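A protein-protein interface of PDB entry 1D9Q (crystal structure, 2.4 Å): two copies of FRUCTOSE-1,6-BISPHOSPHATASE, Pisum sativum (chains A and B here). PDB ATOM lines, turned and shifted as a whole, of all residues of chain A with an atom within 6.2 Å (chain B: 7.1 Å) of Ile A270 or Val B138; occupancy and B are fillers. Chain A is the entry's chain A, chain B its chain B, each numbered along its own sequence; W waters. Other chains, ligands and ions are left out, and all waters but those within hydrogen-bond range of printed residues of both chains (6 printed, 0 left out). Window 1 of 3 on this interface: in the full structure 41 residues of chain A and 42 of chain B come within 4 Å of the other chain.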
ATOM      1  N   LEU A 134     -37.114 -11.421 -11.569  1.00  0.00           N
ATOM      2  CA  LEU A 134     -35.674 -11.586 -11.752  1.00  0.00           C
ATOM      3  C   LEU A 134     -34.874 -10.827 -10.688  1.00  0.00           C
ATOM      4  O   LEU A 134     -33.971 -11.373 -10.061  1.00  0.00           O
ATOM      5  CB  LEU A 134     -35.275 -11.092 -13.154  1.00  0.00           C
ATOM      6  CG  LEU A 134     -33.783 -11.062 -13.516  1.00  0.00           C
ATOM      7  CD1 LEU A 134     -33.296 -12.460 -13.818  1.00  0.00           C
ATOM      8  CD2 LEU A 134     -33.553 -10.159 -14.722  1.00  0.00           C
ATOM      9  N   ASP A 135     -35.224  -9.563 -10.491  1.00  0.00           N
ATOM     10  CA  ASP A 135     -34.550  -8.718  -9.522  1.00  0.00           C
ATOM     11  C   ASP A 135     -34.879  -9.060  -8.082  1.00  0.00           C
ATOM     12  O   ASP A 135     -34.206  -8.596  -7.171  1.00  0.00           O
ATOM     13  CB  ASP A 135     -34.879  -7.249  -9.778  1.00  0.00           C
ATOM     14  CG  ASP A 135     -34.377  -6.757 -11.123  1.00  0.00           C
ATOM     15  OD1 ASP A 135     -33.506  -7.416 -11.735  1.00  0.00           O
ATOM     16  OD2 ASP A 135     -34.853  -5.690 -11.561  1.00  0.00           O
ATOM     17  N   VAL A 138     -33.342 -13.158  -4.974  1.00  0.00           N
ATOM     18  CA  VAL A 138     -32.700 -13.392  -3.672  1.00  0.00           C
ATOM     19  C   VAL A 138     -33.017 -12.352  -2.585  1.00  0.00           C
ATOM     20  O   VAL A 138     -32.882 -12.629  -1.386  1.00  0.00           O
ATOM     21  CB  VAL A 138     -31.149 -13.537  -3.789  1.00  0.00           C
ATOM     22  CG1 VAL A 138     -30.777 -14.768  -4.621  1.00  0.00           C
ATOM     23  CG2 VAL A 138     -30.546 -12.287  -4.370  1.00  0.00           C
ATOM     24  N   SER A 139     -33.445 -11.164  -2.992  1.00  0.00           N
ATOM     25  CA  SER A 139     -33.757 -10.135  -2.021  1.00  0.00           C
ATOM     26  C   SER A 139     -34.666  -9.052  -2.553  1.00  0.00           C
ATOM     27  O   SER A 139     -34.790  -8.851  -3.753  1.00  0.00           O
ATOM     28  CB  SER A 139     -32.479  -9.475  -1.526  1.00  0.00           C
ATOM     29  OG  SER A 139     -31.937  -8.641  -2.528  1.00  0.00           O
ATOM     30  N   MET A 191     -34.867  -4.781   4.675  1.00  0.00           N
ATOM     31  CA  MET A 191     -34.419  -5.710   3.650  1.00  0.00           C
ATOM     32  C   MET A 191     -34.856  -7.127   3.945  1.00  0.00           C
ATOM     33  O   MET A 191     -34.761  -7.593   5.082  1.00  0.00           O
ATOM     34  CB  MET A 191     -32.896  -5.681   3.526  1.00  0.00           C
ATOM     35  CG  MET A 191     -32.355  -6.696   2.533  1.00  0.00           C
ATOM     36  SD  MET A 191     -30.580  -6.682   2.363  1.00  0.00           S
ATOM     37  CE  MET A 191     -30.057  -7.286   3.984  1.00  0.00           C
ATOM     38  N   TYR A 192     -35.347  -7.812   2.922  1.00  0.00           N
ATOM     39  CA  TYR A 192     -35.767  -9.205   3.078  1.00  0.00           C
ATOM     40  C   TYR A 192     -34.806 -10.051   2.253  1.00  0.00           C
ATOM     41  O   TYR A 192     -34.889 -10.074   1.033  1.00  0.00           O
ATOM     42  CB  TYR A 192     -37.200  -9.404   2.571  1.00  0.00           C
ATOM     43  CG  TYR A 192     -38.164  -8.358   3.079  1.00  0.00           C
ATOM     44  CD1 TYR A 192     -38.513  -8.299   4.425  1.00  0.00           C
ATOM     45  CD2 TYR A 192     -38.700  -7.406   2.221  1.00  0.00           C
ATOM     46  CE1 TYR A 192     -39.375  -7.312   4.906  1.00  0.00           C
ATOM     47  CE2 TYR A 192     -39.559  -6.417   2.686  1.00  0.00           C
ATOM     48  CZ  TYR A 192     -39.891  -6.373   4.028  1.00  0.00           C
ATOM     49  OH  TYR A 192     -40.728  -5.381   4.490  1.00  0.00           O
ATOM     50  N   SER A 193     -33.852 -10.688   2.917  1.00  0.00           N
ATOM     51  CA  SER A 193     -32.872 -11.528   2.242  1.00  0.00           C
ATOM     52  C   SER A 193     -32.580 -12.727   3.154  1.00  0.00           C
ATOM     53  O   SER A 193     -33.480 -13.173   3.868  1.00  0.00           O
ATOM     54  CB  SER A 193     -31.601 -10.720   1.940  1.00  0.00           C
ATOM     55  OG  SER A 193     -30.994 -10.230   3.118  1.00  0.00           O
ATOM     56  N   SER A 194     -31.349 -13.255   3.128  1.00  0.00           N
ATOM     57  CA  SER A 194     -30.976 -14.385   3.984  1.00  0.00           C
ATOM     58  C   SER A 194     -31.154 -13.969   5.437  1.00  0.00           C
ATOM     59  O   SER A 194     -31.196 -14.798   6.333  1.00  0.00           O
ATOM     60  CB  SER A 194     -29.533 -14.834   3.730  1.00  0.00           C
ATOM     61  OG  SER A 194     -28.591 -13.836   4.072  1.00  0.00           O
ATOM     62  N   SER A 195     -31.325 -12.664   5.636  1.00  0.00           N
ATOM     63  CA  SER A 195     -31.529 -12.061   6.947  1.00  0.00           C
ATOM     64  C   SER A 195     -32.562 -10.942   6.751  1.00  0.00           C
ATOM     65  O   SER A 195     -32.670 -10.393   5.657  1.00  0.00           O
ATOM     66  CB  SER A 195     -30.206 -11.463   7.424  1.00  0.00           C
ATOM     67  OG  SER A 195     -30.164 -11.343   8.827  1.00  0.00           O
ATOM     68  N   SER A 235     -21.328  -0.851  -8.265  1.00  0.00           N
ATOM     69  CA  SER A 235     -22.590  -1.511  -8.535  1.00  0.00           C
ATOM     70  C   SER A 235     -23.361  -0.767  -9.628  1.00  0.00           C
ATOM     71  O   SER A 235     -24.000   0.245  -9.362  1.00  0.00           O
ATOM     72  CB  SER A 235     -23.386  -1.533  -7.228  1.00  0.00           C
ATOM     73  OG  SER A 235     -24.311  -2.582  -7.184  1.00  0.00           O
ATOM     74  N   ARG A 268     -20.276  -5.847  -8.256  1.00  0.00           N
ATOM     75  CA  ARG A 268     -21.379  -6.564  -7.612  1.00  0.00           C
ATOM     76  C   ARG A 268     -22.673  -5.816  -7.952  1.00  0.00           C
ATOM     77  O   ARG A 268     -22.760  -4.614  -7.734  1.00  0.00           O
ATOM     78  CB  ARG A 268     -21.202  -6.608  -6.081  1.00  0.00           C
ATOM     79  CG  ARG A 268     -20.016  -7.411  -5.569  1.00  0.00           C
ATOM     80  CD  ARG A 268     -20.112  -8.879  -5.947  1.00  0.00           C
ATOM     81  NE  ARG A 268     -19.023  -9.652  -5.354  1.00  0.00           N
ATOM     82  CZ  ARG A 268     -17.800  -9.770  -5.871  1.00  0.00           C
ATOM     83  NH1 ARG A 268     -17.485  -9.173  -7.013  1.00  0.00           N
ATOM     84  NH2 ARG A 268     -16.871 -10.461  -5.226  1.00  0.00           N
ATOM     85  N   TYR A 269     -23.666  -6.524  -8.487  1.00  0.00           N
ATOM     86  CA  TYR A 269     -24.937  -5.918  -8.851  1.00  0.00           C
ATOM     87  C   TYR A 269     -26.039  -6.966  -8.741  1.00  0.00           C
ATOM     88  O   TYR A 269     -26.159  -7.850  -9.577  1.00  0.00           O
ATOM     89  CB  TYR A 269     -24.871  -5.344 -10.283  1.00  0.00           C
ATOM     90  CG  TYR A 269     -26.036  -4.449 -10.632  1.00  0.00           C
ATOM     91  CD1 TYR A 269     -26.132  -3.160 -10.092  1.00  0.00           C
ATOM     92  CD2 TYR A 269     -27.068  -4.892 -11.469  1.00  0.00           C
ATOM     93  CE1 TYR A 269     -27.219  -2.334 -10.374  1.00  0.00           C
ATOM     94  CE2 TYR A 269     -28.165  -4.069 -11.757  1.00  0.00           C
ATOM     95  CZ  TYR A 269     -28.225  -2.793 -11.203  1.00  0.00           C
ATOM     96  OH  TYR A 269     -29.280  -1.964 -11.479  1.00  0.00           O
ATOM     97  N   ILE A 270     -26.840  -6.863  -7.696  1.00  0.00           N
ATOM     98  CA  ILE A 270     -27.925  -7.810  -7.455  1.00  0.00           C
ATOM     99  C   ILE A 270     -29.136  -7.508  -8.339  1.00  0.00           C
ATOM    100  O   ILE A 270     -29.759  -8.415  -8.898  1.00  0.00           O
ATOM    101  CB  ILE A 270     -28.365  -7.760  -5.962  1.00  0.00           C
ATOM    102  CG1 ILE A 270     -27.154  -7.977  -5.059  1.00  0.00           C
ATOM    103  CG2 ILE A 270     -29.442  -8.802  -5.675  1.00  0.00           C
ATOM    104  CD1 ILE A 270     -27.376  -7.610  -3.640  1.00  0.00           C
ATOM    105  N   GLY A 271     -29.449  -6.222  -8.466  1.00  0.00           N
ATOM    106  CA  GLY A 271     -30.590  -5.799  -9.254  1.00  0.00           C
ATOM    107  C   GLY A 271     -31.679  -5.343  -8.305  1.00  0.00           C
ATOM    108  O   GLY A 271     -32.724  -4.860  -8.724  1.00  0.00           O
ATOM    109  N   SER A 272     -31.437  -5.553  -7.014  1.00  0.00           N
ATOM    110  CA  SER A 272     -32.352  -5.162  -5.960  1.00  0.00           C
ATOM    111  C   SER A 272     -31.785  -3.895  -5.356  1.00  0.00           C
ATOM    112  O   SER A 272     -30.673  -3.903  -4.841  1.00  0.00           O
ATOM    113  CB  SER A 272     -32.419  -6.247  -4.893  1.00  0.00           C
ATOM    114  OG  SER A 272     -33.093  -5.771  -3.753  1.00  0.00           O
ATOM    115  N   GLY A 275     -31.110  -4.277  -1.648  1.00  0.00           N
ATOM    116  CA  GLY A 275     -29.992  -5.189  -1.491  1.00  0.00           C
ATOM    117  C   GLY A 275     -28.651  -4.566  -1.852  1.00  0.00           C
ATOM    118  O   GLY A 275     -27.701  -4.655  -1.081  1.00  0.00           O
ATOM    119  N   ASP A 276     -28.570  -3.941  -3.026  1.00  0.00           N
ATOM    120  CA  ASP A 276     -27.336  -3.282  -3.479  1.00  0.00           C
ATOM    121  C   ASP A 276     -26.960  -2.082  -2.597  1.00  0.00           C
ATOM    122  O   ASP A 276     -25.786  -1.791  -2.394  1.00  0.00           O
ATOM    123  CB  ASP A 276     -27.465  -2.823  -4.937  1.00  0.00           C
ATOM    124  CG  ASP A 276     -27.416  -3.974  -5.928  1.00  0.00           C
ATOM    125  OD1 ASP A 276     -26.477  -4.791  -5.866  1.00  0.00           O
ATOM    126  OD2 ASP A 276     -28.309  -4.048  -6.792  1.00  0.00           O
ATOM    127  N   HIS A 278     -27.823  -1.673   0.711  1.00  0.00           N
ATOM    128  CA  HIS A 278     -27.396  -2.196   2.003  1.00  0.00           C
ATOM    129  C   HIS A 278     -25.950  -2.687   1.994  1.00  0.00           C
ATOM    130  O   HIS A 278     -25.190  -2.413   2.917  1.00  0.00           O
ATOM    131  CB  HIS A 278     -28.334  -3.315   2.461  1.00  0.00           C
ATOM    132  CG  HIS A 278     -28.033  -3.827   3.839  1.00  0.00           C
ATOM    133  ND1 HIS A 278     -28.353  -3.123   4.979  1.00  0.00           N
ATOM    134  CD2 HIS A 278     -27.411  -4.954   4.250  1.00  0.00           C
ATOM    135  CE1 HIS A 278     -27.934  -3.796   6.038  1.00  0.00           C
ATOM    136  NE2 HIS A 278     -27.359  -4.908   5.624  1.00  0.00           N
ATOM    137  N   ARG A 279     -25.573  -3.406   0.948  1.00  0.00           N
ATOM    138  CA  ARG A 279     -24.214  -3.917   0.832  1.00  0.00           C
ATOM    139  C   ARG A 279     -23.233  -2.758   0.712  1.00  0.00           C
ATOM    140  O   ARG A 279     -22.128  -2.838   1.226  1.00  0.00           O
ATOM    141  CB  ARG A 279     -24.092  -4.828  -0.387  1.00  0.00           C
ATOM    142  CG  ARG A 279     -22.747  -5.518  -0.546  1.00  0.00           C
ATOM    143  CD  ARG A 279     -22.558  -5.979  -1.992  1.00  0.00           C
ATOM    144  NE  ARG A 279     -22.581  -4.833  -2.901  1.00  0.00           N
ATOM    145  CZ  ARG A 279     -23.418  -4.687  -3.922  1.00  0.00           C
ATOM    146  NH1 ARG A 279     -24.311  -5.621  -4.200  1.00  0.00           N
ATOM    147  NH2 ARG A 279     -23.417  -3.560  -4.617  1.00  0.00           N
ATOM    148  N   VAL B  56     -27.730 -18.725   9.716  1.00  0.00           N
ATOM    149  CA  VAL B  56     -27.508 -17.626   8.779  1.00  0.00           C
ATOM    150  C   VAL B  56     -28.399 -16.419   9.107  1.00  0.00           C
ATOM    151  O   VAL B  56     -27.924 -15.285   9.160  1.00  0.00           O
ATOM    152  CB  VAL B  56     -27.741 -18.109   7.300  1.00  0.00           C
ATOM    153  CG1 VAL B  56     -27.751 -16.942   6.346  1.00  0.00           C
ATOM    154  CG2 VAL B  56     -26.643 -19.084   6.878  1.00  0.00           C
ATOM    155  N   ASN B 133     -17.730 -12.035   3.499  1.00  0.00           N
ATOM    156  CA  ASN B 133     -18.904 -11.356   4.049  1.00  0.00           C
ATOM    157  C   ASN B 133     -19.628 -10.571   2.964  1.00  0.00           C
ATOM    158  O   ASN B 133     -20.855 -10.520   2.933  1.00  0.00           O
ATOM    159  CB  ASN B 133     -18.493 -10.393   5.169  1.00  0.00           C
ATOM    160  CG  ASN B 133     -18.075 -11.106   6.437  1.00  0.00           C
ATOM    161  OD1 ASN B 133     -18.265 -12.309   6.586  1.00  0.00           O
ATOM    162  ND2 ASN B 133     -17.503 -10.359   7.363  1.00  0.00           N
ATOM    163  N   LEU B 134     -18.849  -9.956   2.082  1.00  0.00           N
ATOM    164  CA  LEU B 134     -19.374  -9.164   0.980  1.00  0.00           C
ATOM    165  C   LEU B 134     -20.285  -9.987   0.065  1.00  0.00           C
ATOM    166  O   LEU B 134     -21.378  -9.547  -0.278  1.00  0.00           O
ATOM    167  CB  LEU B 134     -18.211  -8.588   0.164  1.00  0.00           C
ATOM    168  CG  LEU B 134     -18.547  -7.832  -1.120  1.00  0.00           C
ATOM    169  CD1 LEU B 134     -19.017  -6.442  -0.781  1.00  0.00           C
ATOM    170  CD2 LEU B 134     -17.330  -7.770  -2.019  1.00  0.00           C
ATOM    171  N   ASP B 135     -19.822 -11.179  -0.315  1.00  0.00           N
ATOM    172  CA  ASP B 135     -20.565 -12.071  -1.206  1.00  0.00           C
ATOM    173  C   ASP B 135     -21.745 -12.755  -0.538  1.00  0.00           C
ATOM    174  O   ASP B 135     -22.569 -13.368  -1.212  1.00  0.00           O
ATOM    175  CB  ASP B 135     -19.646 -13.142  -1.802  1.00  0.00           C
ATOM    176  CG  ASP B 135     -18.553 -12.567  -2.678  1.00  0.00           C
ATOM    177  OD1 ASP B 135     -18.689 -11.417  -3.140  1.00  0.00           O
ATOM    178  OD2 ASP B 135     -17.554 -13.279  -2.910  1.00  0.00           O
ATOM    179  N   ALA B 136     -21.823 -12.653   0.781  1.00  0.00           N
ATOM    180  CA  ALA B 136     -22.916 -13.276   1.513  1.00  0.00           C
ATOM    181  C   ALA B 136     -23.850 -12.236   2.135  1.00  0.00           C
ATOM    182  O   ALA B 136     -24.635 -12.554   3.033  1.00  0.00           O
ATOM    183  CB  ALA B 136     -22.365 -14.199   2.583  1.00  0.00           C
ATOM    184  N   ALA B 137     -23.789 -11.005   1.632  1.00  0.00           N
ATOM    185  CA  ALA B 137     -24.622  -9.927   2.153  1.00  0.00           C
ATOM    186  C   ALA B 137     -26.131 -10.187   2.040  1.00  0.00           C
ATOM    187  O   ALA B 137     -26.889  -9.837   2.950  1.00  0.00           O
ATOM    188  CB  ALA B 137     -24.246  -8.588   1.486  1.00  0.00           C
ATOM    189  N   VAL B 138     -26.562 -10.802   0.937  1.00  0.00           N
ATOM    190  CA  VAL B 138     -27.984 -11.087   0.731  1.00  0.00           C
ATOM    191  C   VAL B 138     -28.323 -12.569   0.594  1.00  0.00           C
ATOM    192  O   VAL B 138     -29.451 -12.971   0.848  1.00  0.00           O
ATOM    193  CB  VAL B 138     -28.566 -10.323  -0.498  1.00  0.00           C
ATOM    194  CG1 VAL B 138     -28.514  -8.845  -0.253  1.00  0.00           C
ATOM    195  CG2 VAL B 138     -27.813 -10.687  -1.767  1.00  0.00           C
ATOM    196  N   SER B 139     -27.357 -13.379   0.182  1.00  0.00           N
ATOM    197  CA  SER B 139     -27.610 -14.805   0.030  1.00  0.00           C
ATOM    198  C   SER B 139     -26.364 -15.665   0.128  1.00  0.00           C
ATOM    199  O   SER B 139     -25.241 -15.182   0.004  1.00  0.00           O
ATOM    200  CB  SER B 139     -28.309 -15.102  -1.303  1.00  0.00           C
ATOM    201  OG  SER B 139     -27.406 -15.040  -2.391  1.00  0.00           O
ATOM    202  N   THR B 140     -26.601 -16.952   0.367  1.00  0.00           N
ATOM    203  CA  THR B 140     -25.559 -17.965   0.439  1.00  0.00           C
ATOM    204  C   THR B 140     -26.269 -19.323   0.297  1.00  0.00           C
ATOM    205  O   THR B 140     -27.462 -19.361  -0.022  1.00  0.00           O
ATOM    206  CB  THR B 140     -24.698 -17.827   1.727  1.00  0.00           C
ATOM    207  OG1 THR B 140     -23.573 -18.704   1.641  1.00  0.00           O
ATOM    208  CG2 THR B 140     -25.498 -18.125   2.980  1.00  0.00           C
ATOM    209  N   TYR B 192     -30.065 -19.932   0.868  1.00  0.00           N
ATOM    210  CA  TYR B 192     -30.532 -19.149   2.006  1.00  0.00           C
ATOM    211  C   TYR B 192     -30.582 -17.698   1.552  1.00  0.00           C
ATOM    212  O   TYR B 192     -29.549 -17.041   1.417  1.00  0.00           O
ATOM    213  CB  TYR B 192     -29.586 -19.293   3.199  1.00  0.00           C
ATOM    214  CG  TYR B 192     -29.220 -20.725   3.499  1.00  0.00           C
ATOM    215  CD1 TYR B 192     -30.170 -21.629   3.965  1.00  0.00           C
ATOM    216  CD2 TYR B 192     -27.929 -21.185   3.277  1.00  0.00           C
ATOM    217  CE1 TYR B 192     -29.837 -22.967   4.201  1.00  0.00           C
ATOM    218  CE2 TYR B 192     -27.586 -22.507   3.507  1.00  0.00           C
ATOM    219  CZ  TYR B 192     -28.539 -23.395   3.965  1.00  0.00           C
ATOM    220  OH  TYR B 192     -28.190 -24.711   4.166  1.00  0.00           O
ATOM    221  N   SER B 193     -31.781 -17.232   1.232  1.00  0.00           N
ATOM    222  CA  SER B 193     -31.972 -15.858   0.793  1.00  0.00           C
ATOM    223  C   SER B 193     -33.306 -15.363   1.340  1.00  0.00           C
ATOM    224  O   SER B 193     -33.718 -15.789   2.423  1.00  0.00           O
ATOM    225  CB  SER B 193     -31.942 -15.768  -0.730  1.00  0.00           C
ATOM    226  OG  SER B 193     -32.984 -16.533  -1.301  1.00  0.00           O
ATOM    227  N   SER B 194     -33.978 -14.467   0.617  1.00  0.00           N
ATOM    228  CA  SER B 194     -35.271 -13.948   1.071  1.00  0.00           C
ATOM    229  C   SER B 194     -36.242 -15.113   1.223  1.00  0.00           C
ATOM    230  O   SER B 194     -37.272 -15.010   1.882  1.00  0.00           O
ATOM    231  CB  SER B 194     -35.820 -12.916   0.087  1.00  0.00           C
ATOM    232  OG  SER B 194     -36.139 -13.505  -1.154  1.00  0.00           O
ATOM    233  N   ALA B 267     -27.188  -7.395 -17.027  1.00  0.00           N
ATOM    234  CA  ALA B 267     -26.101  -7.913 -16.213  1.00  0.00           C
ATOM    235  C   ALA B 267     -26.558  -8.030 -14.776  1.00  0.00           C
ATOM    236  O   ALA B 267     -27.114  -7.080 -14.224  1.00  0.00           O
ATOM    237  CB  ALA B 267     -24.885  -6.999 -16.298  1.00  0.00           C
ATOM    238  N   ARG B 268     -26.343  -9.205 -14.185  1.00  0.00           N
ATOM    239  CA  ARG B 268     -26.691  -9.485 -12.786  1.00  0.00           C
ATOM    240  C   ARG B 268     -25.595 -10.368 -12.195  1.00  0.00           C
ATOM    241  O   ARG B 268     -25.302 -11.433 -12.734  1.00  0.00           O
ATOM    242  CB  ARG B 268     -28.034 -10.219 -12.671  1.00  0.00           C
ATOM    243  CG  ARG B 268     -29.268  -9.445 -13.124  1.00  0.00           C
ATOM    244  CD  ARG B 268     -29.484  -8.178 -12.312  1.00  0.00           C
ATOM    245  NE  ARG B 268     -30.732  -7.507 -12.680  1.00  0.00           N
ATOM    246  CZ  ARG B 268     -30.875  -6.675 -13.709  1.00  0.00           C
ATOM    247  NH1 ARG B 268     -29.843  -6.383 -14.491  1.00  0.00           N
ATOM    248  NH2 ARG B 268     -32.066  -6.165 -13.980  1.00  0.00           N
ATOM    249  N   TYR B 269     -24.992  -9.922 -11.092  1.00  0.00           N
ATOM    250  CA  TYR B 269     -23.926 -10.672 -10.414  1.00  0.00           C
ATOM    251  C   TYR B 269     -23.953 -10.376  -8.924  1.00  0.00           C
ATOM    252  O   TYR B 269     -23.508  -9.324  -8.486  1.00  0.00           O
ATOM    253  CB  TYR B 269     -22.559 -10.295 -10.978  1.00  0.00           C
ATOM    254  CG  TYR B 269     -21.442 -11.215 -10.568  1.00  0.00           C
ATOM    255  CD1 TYR B 269     -21.317 -12.473 -11.137  1.00  0.00           C
ATOM    256  CD2 TYR B 269     -20.493 -10.826  -9.629  1.00  0.00           C
ATOM    257  CE1 TYR B 269     -20.273 -13.324 -10.785  1.00  0.00           C
ATOM    258  CE2 TYR B 269     -19.443 -11.671  -9.268  1.00  0.00           C
ATOM    259  CZ  TYR B 269     -19.342 -12.922  -9.857  1.00  0.00           C
ATOM    260  OH  TYR B 269     -18.311 -13.776  -9.530  1.00  0.00           O
ATOM    261  N   ILE B 270     -24.494 -11.315  -8.157  1.00  0.00           N
ATOM    262  CA  ILE B 270     -24.604 -11.191  -6.708  1.00  0.00           C
ATOM    263  C   ILE B 270     -23.247 -11.417  -6.029  1.00  0.00           C
ATOM    264  O   ILE B 270     -22.858 -10.679  -5.123  1.00  0.00           O
ATOM    265  CB  ILE B 270     -25.602 -12.235  -6.167  1.00  0.00           C
ATOM    266  CG1 ILE B 270     -26.931 -12.110  -6.896  1.00  0.00           C
ATOM    267  CG2 ILE B 270     -25.806 -12.058  -4.686  1.00  0.00           C
ATOM    268  CD1 ILE B 270     -27.845 -13.264  -6.660  1.00  0.00           C
ATOM    269  N   GLY B 271     -22.531 -12.437  -6.490  1.00  0.00           N
ATOM    270  CA  GLY B 271     -21.241 -12.779  -5.922  1.00  0.00           C
ATOM    271  C   GLY B 271     -21.368 -14.070  -5.143  1.00  0.00           C
ATOM    272  O   GLY B 271     -20.385 -14.622  -4.676  1.00  0.00           O
ATOM    273  N   SER B 272     -22.613 -14.509  -4.967  1.00  0.00           N
ATOM    274  CA  SER B 272     -22.968 -15.744  -4.277  1.00  0.00           C
ATOM    275  C   SER B 272     -23.180 -16.806  -5.355  1.00  0.00           C
ATOM    276  O   SER B 272     -24.091 -16.679  -6.177  1.00  0.00           O
ATOM    277  CB  SER B 272     -24.276 -15.530  -3.505  1.00  0.00           C
ATOM    278  OG  SER B 272     -24.813 -16.746  -3.019  1.00  0.00           O
ATOM    279  N   ASP B 276     -26.474 -16.769  -7.681  1.00  0.00           N
ATOM    280  CA  ASP B 276     -26.338 -16.519  -9.108  1.00  0.00           C
ATOM    281  C   ASP B 276     -26.750 -17.724  -9.940  1.00  0.00           C
ATOM    282  O   ASP B 276     -27.351 -17.561 -11.002  1.00  0.00           O
ATOM    283  CB  ASP B 276     -24.900 -16.124  -9.451  1.00  0.00           C
ATOM    284  CG  ASP B 276     -24.571 -14.715  -9.027  1.00  0.00           C
ATOM    285  OD1 ASP B 276     -25.369 -13.812  -9.339  1.00  0.00           O
ATOM    286  OD2 ASP B 276     -23.528 -14.501  -8.377  1.00  0.00           O
ATOM    287  N   ARG B 279     -30.722 -18.192  -9.882  1.00  0.00           N
ATOM    288  CA  ARG B 279     -31.378 -17.213 -10.729  1.00  0.00           C
ATOM    289  C   ARG B 279     -31.223 -17.638 -12.183  1.00  0.00           C
ATOM    290  O   ARG B 279     -32.147 -17.486 -12.976  1.00  0.00           O
ATOM    291  CB  ARG B 279     -30.760 -15.837 -10.523  1.00  0.00           C
ATOM    292  CG  ARG B 279     -31.476 -14.716 -11.253  1.00  0.00           C
ATOM    293  CD  ARG B 279     -30.572 -13.492 -11.382  1.00  0.00           C
ATOM    294  NE  ARG B 279     -29.356 -13.829 -12.113  1.00  0.00           N
ATOM    295  CZ  ARG B 279     -28.124 -13.730 -11.618  1.00  0.00           C
ATOM    296  NH1 ARG B 279     -27.927 -13.276 -10.389  1.00  0.00           N
ATOM    297  NH2 ARG B 279     -27.088 -14.156 -12.327  1.00  0.00           N
HETATM  298  O   HOH W   1     -23.977  -8.242  -3.976  1.00  0.00           O
HETATM  299  O   HOH W   2     -28.278 -11.146   5.096  1.00  0.00           O
HETATM  300  O   HOH W   3     -29.926 -11.091  -9.116  1.00  0.00           O
HETATM  301  O   HOH W   4     -32.758 -17.499   5.051  1.00  0.00           O
HETATM  302  O   HOH W   5     -26.220 -14.732   3.855  1.00  0.00           O
HETATM  303  O   HOH W   6     -26.318  -8.014   5.163  1.00  0.00           O
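Val A138 touches Ile B270, and with the chains exchanged Ile A270 touches Val B138. Tyr A192 touches Ser B194, and with the chains exchanged Ser A194 touches Tyr B192. Ser A193 touches its own counterpart, Ser B193. Arg A268 touches Gly B271, and with the chains exchanged Gly A271 touches Arg B268. Of the 27 pairs that touch across the chains among the printed residues, 23 have their exchanged pair printed and touching as well.
The backbone carbonyl oxygen (O) of Val B138 sits at hydrogen-bond distance from the backbone NH (N) of Ser A194 (3.0 Å). NE of Arg A268 is in salt-bridge range of OD1 of Asp B135 (2.9 Å). The backbone carbonyl oxygen of Ser A193 sits close to the backbone carbonyl oxygen of Ser B193 (3.0 Å). N of Tyr A269 lies within hydrogen-bond range of O of Tyr B269 (2.8 Å). The guanidinium group (NE) of Arg B268 lies within salt-bridge range of the side-chain carboxylate (OD1) of Asp A135 (2.9 Å). The backbone carbonyl oxygen (O) of Val A138 lies within hydrogen-bond range of the backbone NH (N) of Ser B194 (2.9 Å).
Of the 20 printed residues of chain B, 14 touch a printed residue of chain A. Printed residues of chain B that touch a printed residue of chain A: Val B56, Leu B134, Asp B135, Ala B137, Val B138, Tyr B192, Ser B193, Ser B194, Ala B267, Arg B268, Tyr B269, Ile B270, Gly B271 and Arg B279. Hydrophobic or aromatic side chains of chain B within 4 Å of the printed part of chain A: Val B56, Leu B134, Ala B137, Val B138, Tyr B269 and Ile B270. Of the 19 printed residues of chain A, 12 touch a printed residue of chain B. Among the printed residues, Asp or Glu carboxylates within 4 Å of a Lys or Arg side-chain nitrogen of the other chain: Asp A135 with Arg B268 and Arg A268 with Asp B135.
CD1 of Ile B270 touches CG2 of Val A138, 3.7 Å away. SD of Met A191 touches CG1 of Val B138 (3.97 Å). CB of Ser A193 touches O of Val B138, 3.3 Å away. Ser A194 touches Tyr B192 (CB to O, 3.2 Å). Ser A194 touches Ser B193. Ser A194 touches Ser B194. O of Tyr B269 touches CA of Arg A268, at 3.6 Å. O of Ile B270 touches CD of Arg A268, 3.4 Å away. CD1 of Ile A270 touches CG2 of Val B138, at 3.6 Å. Ala B137 touches Arg A279 (CB to CG, 3.98 Å).
Water W3 bridges the backbone carbonyl oxygen (O) of Ile A270 (2.7 Å) and the guanidinium group (NH1) of Arg B279 (3.2 Å). Water W6 lies within hydrogen-bond range of O of Ala B137 (2.9 Å) and NE2 of His A278 (3.3 Å). Water W4 lies within hydrogen-bond range of the backbone carbonyl oxygen (O) of Ser B193 and the backbone carbonyl oxygen (O) of Ser A194.
Of chain B, only Val B138 (3.6 Å) and Arg B268 (3.4 Å) come within 4 Å of Ile A270. Val B138 touches just these residues of chain A: Met A191 (3.97 Å), Ser A193 (3.3 Å), Ser A194 (3.0 Å) and Ile A270 (3.6 Å). Of the printed residues of chain A, Gly B271 touches Arg A268. Of the printed residues of chain A, Ser B193 touches Val A138 (3.3 Å), Ser A193 (3.0 Å) and Ser A194 (3.4 Å). Asp A276 touches none of the printed residues of chain B. The nearest residue of chain B that does not touch Ile A270 is Tyr B269 (4.2 Å). The nearest printed residue of chain A that does not touch Ser B194 is Ser A139 (4.01 Å).
The guanidinium group (NH2) of Arg B279 is in hydrogen-bond range of the backbone carbonyl oxygen (O) of Arg B268 (3.3 Å). The side-chain hydroxyl (OG) of Ser A193 lies close to the side-chain sulfur (SD) of Met A191 (3.7 Å). The guanidinium group (NH1) of Arg A279 is in salt-bridge range of the side-chain carboxylate (OD1) of Asp A276 (2.9 Å).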
